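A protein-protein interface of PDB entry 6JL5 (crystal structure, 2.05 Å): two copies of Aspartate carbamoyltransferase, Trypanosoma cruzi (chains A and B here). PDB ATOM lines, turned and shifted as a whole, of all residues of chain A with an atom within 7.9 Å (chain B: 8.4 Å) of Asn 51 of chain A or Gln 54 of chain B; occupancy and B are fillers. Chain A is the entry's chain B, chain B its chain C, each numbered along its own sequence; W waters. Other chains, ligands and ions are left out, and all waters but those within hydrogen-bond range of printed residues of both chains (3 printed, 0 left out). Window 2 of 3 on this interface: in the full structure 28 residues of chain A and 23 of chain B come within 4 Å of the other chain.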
ATOM      1  N   LEU A   8      10.501  28.127  -0.653  1.00  0.00           N
ATOM      2  CA  LEU A   8      10.428  28.785   0.651  1.00  0.00           C
ATOM      3  C   LEU A   8       9.626  30.065   0.504  1.00  0.00           C
ATOM      4  O   LEU A   8      10.198  31.152   0.569  1.00  0.00           O
ATOM      5  CB  LEU A   8      11.841  29.080   1.171  1.00  0.00           C
ATOM      6  CG  LEU A   8      12.746  27.863   1.372  1.00  0.00           C
ATOM      7  CD1 LEU A   8      14.127  28.263   1.806  1.00  0.00           C
ATOM      8  CD2 LEU A   8      12.136  26.884   2.389  1.00  0.00           C
ATOM      9  N   GLY A  47      21.693  19.736   4.503  1.00  0.00           N
ATOM     10  CA  GLY A  47      22.995  20.370   4.305  1.00  0.00           C
ATOM     11  C   GLY A  47      23.004  21.511   3.312  1.00  0.00           C
ATOM     12  O   GLY A  47      24.072  22.027   2.947  1.00  0.00           O
ATOM     13  N   GLU A  48      21.818  21.905   2.859  1.00  0.00           N
ATOM     14  CA  GLU A  48      21.675  23.027   1.943  1.00  0.00           C
ATOM     15  C   GLU A  48      21.989  24.347   2.646  1.00  0.00           C
ATOM     16  O   GLU A  48      21.661  24.529   3.825  1.00  0.00           O
ATOM     17  CB  GLU A  48      20.263  23.078   1.350  1.00  0.00           C
ATOM     18  CG  GLU A  48      20.186  23.996   0.141  1.00  0.00           C
ATOM     19  CD  GLU A  48      18.825  24.026  -0.547  1.00  0.00           C
ATOM     20  OE1 GLU A  48      18.180  22.959  -0.707  1.00  0.00           O
ATOM     21  OE2 GLU A  48      18.417  25.138  -0.949  1.00  0.00           O
ATOM     22  N   VAL A  49      22.625  25.251   1.903  1.00  0.00           N
ATOM     23  CA  VAL A  49      23.052  26.551   2.395  1.00  0.00           C
ATOM     24  C   VAL A  49      22.062  27.560   1.834  1.00  0.00           C
ATOM     25  O   VAL A  49      21.857  27.603   0.607  1.00  0.00           O
ATOM     26  CB  VAL A  49      24.478  26.889   1.902  1.00  0.00           C
ATOM     27  CG1 VAL A  49      24.836  28.351   2.194  1.00  0.00           C
ATOM     28  CG2 VAL A  49      25.486  25.941   2.506  1.00  0.00           C
ATOM     29  N   LEU A  50      21.416  28.330   2.717  1.00  0.00           N
ATOM     30  CA  LEU A  50      20.478  29.363   2.275  1.00  0.00           C
ATOM     31  C   LEU A  50      21.164  30.730   2.306  1.00  0.00           C
ATOM     32  O   LEU A  50      21.899  31.029   3.247  1.00  0.00           O
ATOM     33  CB  LEU A  50      19.207  29.365   3.138  1.00  0.00           C
ATOM     34  CG  LEU A  50      18.467  28.048   3.439  1.00  0.00           C
ATOM     35  CD1 LEU A  50      17.341  28.275   4.390  1.00  0.00           C
ATOM     36  CD2 LEU A  50      17.941  27.387   2.157  1.00  0.00           C
ATOM     37  N   ASN A  51      20.937  31.540   1.267  1.00  0.00           N
ATOM     38  CA  ASN A  51      21.436  32.908   1.199  1.00  0.00           C
ATOM     39  C   ASN A  51      20.330  33.936   0.993  1.00  0.00           C
ATOM     40  O   ASN A  51      20.512  34.922   0.273  1.00  0.00           O
ATOM     41  CB  ASN A  51      22.548  33.058   0.138  1.00  0.00           C
ATOM     42  CG  ASN A  51      23.934  33.174   0.772  1.00  0.00           C
ATOM     43  OD1 ASN A  51      24.127  33.899   1.761  1.00  0.00           O
ATOM     44  ND2 ASN A  51      24.896  32.437   0.228  1.00  0.00           N
ATOM     45  N   LEU A  52      19.203  33.727   1.664  1.00  0.00           N
ATOM     46  CA  LEU A  52      18.027  34.575   1.526  1.00  0.00           C
ATOM     47  C   LEU A  52      18.215  35.976   2.080  1.00  0.00           C
ATOM     48  O   LEU A  52      17.751  36.934   1.475  1.00  0.00           O
ATOM     49  CB  LEU A  52      16.824  33.906   2.194  1.00  0.00           C
ATOM     50  CG  LEU A  52      16.441  32.556   1.556  1.00  0.00           C
ATOM     51  CD1 LEU A  52      15.374  31.842   2.370  1.00  0.00           C
ATOM     52  CD2 LEU A  52      15.977  32.770   0.122  1.00  0.00           C
ATOM     53  N   LEU A  53      18.912  36.106   3.220  1.00  0.00           N
ATOM     54  CA  LEU A  53      19.075  37.430   3.831  1.00  0.00           C
ATOM     55  C   LEU A  53      20.504  37.961   3.839  1.00  0.00           C
ATOM     56  O   LEU A  53      20.897  38.676   4.773  1.00  0.00           O
ATOM     57  CB  LEU A  53      18.478  37.461   5.246  1.00  0.00           C
ATOM     58  CG  LEU A  53      16.992  37.131   5.351  1.00  0.00           C
ATOM     59  CD1 LEU A  53      16.595  36.989   6.827  1.00  0.00           C
ATOM     60  CD2 LEU A  53      16.172  38.235   4.684  1.00  0.00           C
ATOM     61  N   GLN A  54      21.275  37.642   2.802  1.00  0.00           N
ATOM     62  CA  GLN A  54      22.623  38.185   2.672  1.00  0.00           C
ATOM     63  C   GLN A  54      22.572  39.697   2.753  1.00  0.00           C
ATOM     64  O   GLN A  54      21.690  40.335   2.172  1.00  0.00           O
ATOM     65  CB  GLN A  54      23.277  37.786   1.350  1.00  0.00           C
ATOM     66  CG  GLN A  54      24.793  38.007   1.388  1.00  0.00           C
ATOM     67  CD  GLN A  54      25.515  37.493   0.127  1.00  0.00           C
ATOM     68  OE1 GLN A  54      24.965  36.717  -0.655  1.00  0.00           O
ATOM     69  NE2 GLN A  54      26.752  37.932  -0.057  1.00  0.00           N
ATOM     70  N   GLY A  55      23.522  40.269   3.474  1.00  0.00           N
ATOM     71  CA  GLY A  55      23.546  41.709   3.651  1.00  0.00           C
ATOM     72  C   GLY A  55      22.479  42.322   4.556  1.00  0.00           C
ATOM     73  O   GLY A  55      22.405  43.559   4.644  1.00  0.00           O
ATOM     74  N   ILE A  78      21.625  33.756  10.912  1.00  0.00           N
ATOM     75  CA  ILE A  78      22.803  33.233  10.230  1.00  0.00           C
ATOM     76  C   ILE A  78      22.446  32.129   9.201  1.00  0.00           C
ATOM     77  O   ILE A  78      22.895  32.187   8.058  1.00  0.00           O
ATOM     78  CB  ILE A  78      23.860  32.741  11.233  1.00  0.00           C
ATOM     79  CG1 ILE A  78      24.477  33.956  11.969  1.00  0.00           C
ATOM     80  CG2 ILE A  78      24.944  31.869  10.475  1.00  0.00           C
ATOM     81  CD1 ILE A  78      25.108  33.640  13.334  1.00  0.00           C
ATOM     82  N   ARG A  79      21.590  31.181   9.584  1.00  0.00           N
ATOM     83  CA  ARG A  79      21.221  30.095   8.682  1.00  0.00           C
ATOM     84  C   ARG A  79      20.340  30.539   7.494  1.00  0.00           C
ATOM     85  O   ARG A  79      20.106  29.770   6.544  1.00  0.00           O
ATOM     86  CB  ARG A  79      20.560  28.962   9.455  1.00  0.00           C
ATOM     87  CG  ARG A  79      21.519  28.255  10.395  1.00  0.00           C
ATOM     88  CD  ARG A  79      20.927  26.915  10.853  1.00  0.00           C
ATOM     89  NE  ARG A  79      21.811  26.272  11.817  1.00  0.00           N
ATOM     90  CZ  ARG A  79      22.827  25.472  11.501  1.00  0.00           C
ATOM     91  NH1 ARG A  79      23.084  25.201  10.226  1.00  0.00           N
ATOM     92  NH2 ARG A  79      23.560  24.900  12.457  1.00  0.00           N
ATOM     93  N   LEU A  80      19.857  31.780   7.544  1.00  0.00           N
ATOM     94  CA  LEU A  80      19.220  32.402   6.385  1.00  0.00           C
ATOM     95  C   LEU A  80      20.217  33.206   5.529  1.00  0.00           C
ATOM     96  O   LEU A  80      19.818  33.850   4.534  1.00  0.00           O
ATOM     97  CB  LEU A  80      18.093  33.312   6.845  1.00  0.00           C
ATOM     98  CG  LEU A  80      16.798  32.642   7.311  1.00  0.00           C
ATOM     99  CD1 LEU A  80      15.934  33.648   8.072  1.00  0.00           C
ATOM    100  CD2 LEU A  80      15.986  32.015   6.153  1.00  0.00           C
ATOM    101  N   GLY A  81      21.501  33.150   5.881  1.00  0.00           N
ATOM    102  CA  GLY A  81      22.508  34.005   5.213  1.00  0.00           C
ATOM    103  C   GLY A  81      22.625  35.431   5.758  1.00  0.00           C
ATOM    104  O   GLY A  81      23.437  36.235   5.271  1.00  0.00           O
ATOM    105  N   GLY A  82      21.800  35.750   6.748  1.00  0.00           N
ATOM    106  CA  GLY A  82      21.850  37.025   7.452  1.00  0.00           C
ATOM    107  C   GLY A  82      23.050  37.220   8.388  1.00  0.00           C
ATOM    108  O   GLY A  82      23.853  36.305   8.592  1.00  0.00           O
ATOM    109  N   TRP A 326      12.605  35.363   7.730  1.00  0.00           N
ATOM    110  CA  TRP A 326      12.480  35.427   6.264  1.00  0.00           C
ATOM    111  C   TRP A 326      11.170  36.141   5.851  1.00  0.00           C
ATOM    112  O   TRP A 326      11.152  37.047   4.993  1.00  0.00           O
ATOM    113  CB  TRP A 326      12.555  34.003   5.680  1.00  0.00           C
ATOM    114  CG  TRP A 326      12.307  33.871   4.184  1.00  0.00           C
ATOM    115  CD1 TRP A 326      11.508  32.932   3.574  1.00  0.00           C
ATOM    116  CD2 TRP A 326      12.831  34.694   3.125  1.00  0.00           C
ATOM    117  NE1 TRP A 326      11.525  33.106   2.214  1.00  0.00           N
ATOM    118  CE2 TRP A 326      12.327  34.175   1.906  1.00  0.00           C
ATOM    119  CE3 TRP A 326      13.700  35.792   3.081  1.00  0.00           C
ATOM    120  CZ2 TRP A 326      12.648  34.731   0.660  1.00  0.00           C
ATOM    121  CZ3 TRP A 326      14.021  36.346   1.829  1.00  0.00           C
ATOM    122  CH2 TRP A 326      13.503  35.808   0.645  1.00  0.00           C
ATOM    123  N   LEU B  50      38.213  31.450   1.329  1.00  0.00           N
ATOM    124  CA  LEU B  50      37.623  30.117   1.431  1.00  0.00           C
ATOM    125  C   LEU B  50      36.119  30.149   1.744  1.00  0.00           C
ATOM    126  O   LEU B  50      35.638  31.030   2.446  1.00  0.00           O
ATOM    127  CB  LEU B  50      38.400  29.305   2.461  1.00  0.00           C
ATOM    128  CG  LEU B  50      39.922  29.256   2.216  1.00  0.00           C
ATOM    129  CD1 LEU B  50      40.644  28.538   3.357  1.00  0.00           C
ATOM    130  CD2 LEU B  50      40.224  28.573   0.871  1.00  0.00           C
ATOM    131  N   ASN B  51      35.370  29.204   1.200  1.00  0.00           N
ATOM    132  CA  ASN B  51      33.936  29.131   1.451  1.00  0.00           C
ATOM    133  C   ASN B  51      33.495  27.745   1.907  1.00  0.00           C
ATOM    134  O   ASN B  51      32.286  27.420   1.891  1.00  0.00           O
ATOM    135  CB  ASN B  51      33.107  29.621   0.237  1.00  0.00           C
ATOM    136  CG  ASN B  51      32.217  30.820   0.569  1.00  0.00           C
ATOM    137  OD1 ASN B  51      31.921  31.641  -0.311  1.00  0.00           O
ATOM    138  ND2 ASN B  51      31.779  30.935   1.846  1.00  0.00           N
ATOM    139  N   LEU B  52      34.479  26.971   2.355  1.00  0.00           N
ATOM    140  CA  LEU B  52      34.335  25.590   2.800  1.00  0.00           C
ATOM    141  C   LEU B  52      33.210  25.251   3.795  1.00  0.00           C
ATOM    142  O   LEU B  52      32.606  24.199   3.664  1.00  0.00           O
ATOM    143  CB  LEU B  52      35.677  25.085   3.329  1.00  0.00           C
ATOM    144  CG  LEU B  52      36.849  25.043   2.315  1.00  0.00           C
ATOM    145  CD1 LEU B  52      38.105  24.475   2.928  1.00  0.00           C
ATOM    146  CD2 LEU B  52      36.506  24.241   1.051  1.00  0.00           C
ATOM    147  N   LEU B  53      32.954  26.119   4.787  1.00  0.00           N
ATOM    148  CA  LEU B  53      31.979  25.832   5.851  1.00  0.00           C
ATOM    149  C   LEU B  53      30.854  26.872   5.901  1.00  0.00           C
ATOM    150  O   LEU B  53      30.319  27.197   6.987  1.00  0.00           O
ATOM    151  CB  LEU B  53      32.660  25.742   7.233  1.00  0.00           C
ATOM    152  CG  LEU B  53      33.703  24.623   7.452  1.00  0.00           C
ATOM    153  CD1 LEU B  53      34.189  24.668   8.900  1.00  0.00           C
ATOM    154  CD2 LEU B  53      33.085  23.273   7.157  1.00  0.00           C
ATOM    155  N   GLN B  54      30.519  27.403   4.732  1.00  0.00           N
ATOM    156  CA  GLN B  54      29.432  28.340   4.631  1.00  0.00           C
ATOM    157  C   GLN B  54      28.170  27.658   5.152  1.00  0.00           C
ATOM    158  O   GLN B  54      27.936  26.495   4.846  1.00  0.00           O
ATOM    159  CB  GLN B  54      29.256  28.823   3.198  1.00  0.00           C
ATOM    160  CG  GLN B  54      28.288  30.049   3.087  1.00  0.00           C
ATOM    161  CD  GLN B  54      27.829  30.328   1.640  1.00  0.00           C
ATOM    162  OE1 GLN B  54      28.397  29.802   0.656  1.00  0.00           O
ATOM    163  NE2 GLN B  54      26.793  31.155   1.510  1.00  0.00           N
ATOM    164  N   GLY B  55      27.384  28.377   5.965  1.00  0.00           N
ATOM    165  CA  GLY B  55      26.174  27.830   6.538  1.00  0.00           C
ATOM    166  C   GLY B  55      26.369  26.986   7.789  1.00  0.00           C
ATOM    167  O   GLY B  55      25.397  26.505   8.344  1.00  0.00           O
ATOM    168  N   ARG B  56      27.609  26.803   8.250  1.00  0.00           N
ATOM    169  CA  ARG B  56      27.864  26.008   9.467  1.00  0.00           C
ATOM    170  C   ARG B  56      28.181  26.903  10.676  1.00  0.00           C
ATOM    171  O   ARG B  56      28.784  27.947  10.518  1.00  0.00           O
ATOM    172  CB  ARG B  56      28.993  25.006   9.244  1.00  0.00           C
ATOM    173  CG  ARG B  56      28.898  24.223   7.904  1.00  0.00           C
ATOM    174  CD  ARG B  56      27.857  23.129   7.898  1.00  0.00           C
ATOM    175  NE  ARG B  56      27.646  22.703   6.509  1.00  0.00           N
ATOM    176  CZ  ARG B  56      26.485  22.774   5.843  1.00  0.00           C
ATOM    177  NH1 ARG B  56      25.373  23.204   6.437  1.00  0.00           N
ATOM    178  NH2 ARG B  56      26.428  22.384   4.570  1.00  0.00           N
ATOM    179  N   ILE B  57      27.773  26.489  11.876  1.00  0.00           N
ATOM    180  CA  ILE B  57      27.867  27.371  13.049  1.00  0.00           C
ATOM    181  C   ILE B  57      28.758  26.780  14.146  1.00  0.00           C
ATOM    182  O   ILE B  57      28.574  25.625  14.542  1.00  0.00           O
ATOM    183  CB  ILE B  57      26.470  27.707  13.622  1.00  0.00           C
ATOM    184  CG1 ILE B  57      25.678  28.620  12.658  1.00  0.00           C
ATOM    185  CG2 ILE B  57      26.585  28.331  15.074  1.00  0.00           C
ATOM    186  CD1 ILE B  57      24.215  28.906  13.098  1.00  0.00           C
ATOM    187  N   MET B  77      37.166  29.870  12.112  1.00  0.00           N
ATOM    188  CA  MET B  77      35.834  29.488  11.594  1.00  0.00           C
ATOM    189  C   MET B  77      35.439  30.422  10.469  1.00  0.00           C
ATOM    190  O   MET B  77      35.016  29.997   9.390  1.00  0.00           O
ATOM    191  CB  MET B  77      34.783  29.513  12.716  1.00  0.00           C
ATOM    192  CG  MET B  77      33.439  28.976  12.278  1.00  0.00           C
ATOM    193  SD  MET B  77      33.487  27.195  11.944  1.00  0.00           S
ATOM    194  CE  MET B  77      31.754  26.889  11.557  1.00  0.00           C
ATOM    195  N   ILE B  78      35.547  31.714  10.746  1.00  0.00           N
ATOM    196  CA  ILE B  78      35.232  32.758   9.774  1.00  0.00           C
ATOM    197  C   ILE B  78      36.030  32.624   8.460  1.00  0.00           C
ATOM    198  O   ILE B  78      35.461  32.758   7.374  1.00  0.00           O
ATOM    199  CB  ILE B  78      35.404  34.159  10.416  1.00  0.00           C
ATOM    200  CG1 ILE B  78      34.158  34.488  11.281  1.00  0.00           C
ATOM    201  CG2 ILE B  78      35.638  35.264   9.343  1.00  0.00           C
ATOM    202  CD1 ILE B  78      34.411  35.616  12.295  1.00  0.00           C
ATOM    203  N   LEU B  80      37.231  30.068   7.111  1.00  0.00           N
ATOM    204  CA  LEU B  80      36.743  28.923   6.357  1.00  0.00           C
ATOM    205  C   LEU B  80      35.390  29.211   5.729  1.00  0.00           C
ATOM    206  O   LEU B  80      34.848  28.368   5.025  1.00  0.00           O
ATOM    207  CB  LEU B  80      36.642  27.682   7.253  1.00  0.00           C
ATOM    208  CG  LEU B  80      38.013  27.108   7.673  1.00  0.00           C
ATOM    209  CD1 LEU B  80      37.840  26.030   8.732  1.00  0.00           C
ATOM    210  CD2 LEU B  80      38.790  26.546   6.439  1.00  0.00           C
ATOM    211  N   GLY B  81      34.836  30.386   5.994  1.00  0.00           N
ATOM    212  CA  GLY B  81      33.523  30.753   5.461  1.00  0.00           C
ATOM    213  C   GLY B  81      32.382  30.444   6.417  1.00  0.00           C
ATOM    214  O   GLY B  81      31.228  30.679   6.094  1.00  0.00           O
ATOM    215  N   GLY B  82      32.713  29.926   7.602  1.00  0.00           N
ATOM    216  CA  GLY B  82      31.707  29.566   8.616  1.00  0.00           C
ATOM    217  C   GLY B  82      31.222  30.757   9.442  1.00  0.00           C
ATOM    218  O   GLY B  82      31.642  31.885   9.245  1.00  0.00           O
ATOM    219  N   SER B  83      30.345  30.478  10.391  1.00  0.00           N
ATOM    220  CA  SER B  83      29.730  31.491  11.204  1.00  0.00           C
ATOM    221  C   SER B  83      29.850  31.142  12.697  1.00  0.00           C
ATOM    222  O   SER B  83      30.075  29.984  13.072  1.00  0.00           O
ATOM    223  CB  SER B  83      28.276  31.652  10.813  1.00  0.00           C
ATOM    224  OG  SER B  83      28.188  32.085   9.465  1.00  0.00           O
ATOM    225  N   ASP B 112      26.777  23.455  14.789  1.00  0.00           N
ATOM    226  CA  ASP B 112      27.450  22.323  14.131  1.00  0.00           C
ATOM    227  C   ASP B 112      28.628  21.808  14.962  1.00  0.00           C
ATOM    228  O   ASP B 112      29.007  20.641  14.867  1.00  0.00           O
ATOM    229  CB  ASP B 112      27.914  22.740  12.729  1.00  0.00           C
ATOM    230  CG  ASP B 112      26.741  23.013  11.812  1.00  0.00           C
ATOM    231  OD1 ASP B 112      26.234  22.044  11.236  1.00  0.00           O
ATOM    232  OD2 ASP B 112      26.264  24.175  11.717  1.00  0.00           O
ATOM    233  N   TRP B 326      37.874  22.258   9.668  1.00  0.00           N
ATOM    234  CA  TRP B 326      37.558  21.756   8.338  1.00  0.00           C
ATOM    235  C   TRP B 326      37.492  20.243   8.367  1.00  0.00           C
ATOM    236  O   TRP B 326      36.546  19.675   7.866  1.00  0.00           O
ATOM    237  CB  TRP B 326      38.579  22.262   7.314  1.00  0.00           C
ATOM    238  CG  TRP B 326      38.440  21.643   5.927  1.00  0.00           C
ATOM    239  CD1 TRP B 326      39.455  21.120   5.164  1.00  0.00           C
ATOM    240  CD2 TRP B 326      37.232  21.471   5.154  1.00  0.00           C
ATOM    241  NE1 TRP B 326      38.960  20.640   3.971  1.00  0.00           N
ATOM    242  CE2 TRP B 326      37.603  20.833   3.936  1.00  0.00           C
ATOM    243  CE3 TRP B 326      35.873  21.788   5.365  1.00  0.00           C
ATOM    244  CZ2 TRP B 326      36.668  20.518   2.936  1.00  0.00           C
ATOM    245  CZ3 TRP B 326      34.943  21.459   4.369  1.00  0.00           C
ATOM    246  CH2 TRP B 326      35.343  20.853   3.168  1.00  0.00           C
HETATM  247  O   HOH W   1      24.503  22.944   9.622  1.00  0.00           O
HETATM  248  O   HOH W   2      22.646  23.659   5.939  1.00  0.00           O
HETATM  249  O   HOH W   3      23.016  26.239   7.337  1.00  0.00           O
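The side-chain amide nitrogen (ND2) of Asn 51 of chain A sits close to the side-chain amide nitrogen (NE2) of Gln 54 of chain B, at 2.6 Å.
NH2 of Arg 56 of chain B lies within hydrogen-bond range of O of Gly 47 of chain A (2.9 Å).
The guanidinium group of Arg 79 of chain A lies within salt-bridge range of the side-chain carboxylate of Asp 112 of chain B (2.9 Å).
NH1 of Arg 79 of chain A lies within hydrogen-bond range of O of Gly 55 of chain B.
The backbone carbonyl oxygen of Arg 56 of chain B lies within hydrogen-bond range of the backbone NH of Ser 83 of chain B, at 3.0 Å.
OD2 of Asp 112 of chain B is in hydrogen-bond range of N of Ile 57 of chain B, 2.8 Å away.
Val 49 of chain A touches Gln 54 of chain B (CG2 to O, 3.4 Å).
Ile 57 of chain B touches Ile 78 of chain A.
CB of Ser 83 of chain B touches CG2 of Ile 78 of chain A (3.4 Å).
Ile 57 of chain B touches Arg 79 of chain A (CD1 to NE, 3.8 Å).
Of the printed residues of chain B, Gly 47 of chain A touches Arg 56.
Of the printed residues of chain B, Val 49 of chain A touches Gln 54.
Leu 50 of chain A touches none of the printed residues of chain B.
Asn 51 of chain A touches one residue of chain B.
Of the printed residues of chain A, Gln 54 of chain B touches Val 49 and Asn 51.
Printed residues of chain A within 4 Å of Arg 56 of chain B: Gly 47 (2.9 Å).
Gly 82 of chain B touches none of the printed residues of chain A.
The nearest residue of chain B that does not touch Asn 51 of chain A is Asn 51 of chain B (7.1 Å).
Of the 16 printed residues of chain B, 6 touch a printed residue of chain A.
Hydrophobic or aromatic side chains of chain B within 4 Å of the printed part of chain A: Ile 57.
Along chain B the printed residues that touch a printed residue of chain A span positions 54 to 112.
Hydrophobic or aromatic side chains of chain A within 4 Å of the printed part of chain B: Val 49 and Ile 78.
Among the printed residues, 8 pairs touch across the chains.
Asn 51 of chain A touches Gln 54 of chain B, but with the chains exchanged Gln 54 of chain A does not touch Asn 51 of chain B (8.1 Å).
Positions printed for both chains: 50, 51, 52, 53, 54, 55, 78, 80, 81, 82 and 326.
Water W2 lies within hydrogen-bond range of O of Glu 48 of chain A and NH1 of Arg 56 of chain B.
Water W1 lies within hydrogen-bond range of the side-chain carboxylate (OD1) of Asp 112 of chain B, the guanidinium group (NH1) of Arg 79 of chain A and the guanidinium group (NH1) of Arg 56 of chain B.
Water W3 bridges O of Gly 55 of chain B (2.6 Å) and NH1 of Arg 79 of chain A (3.1 Å).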
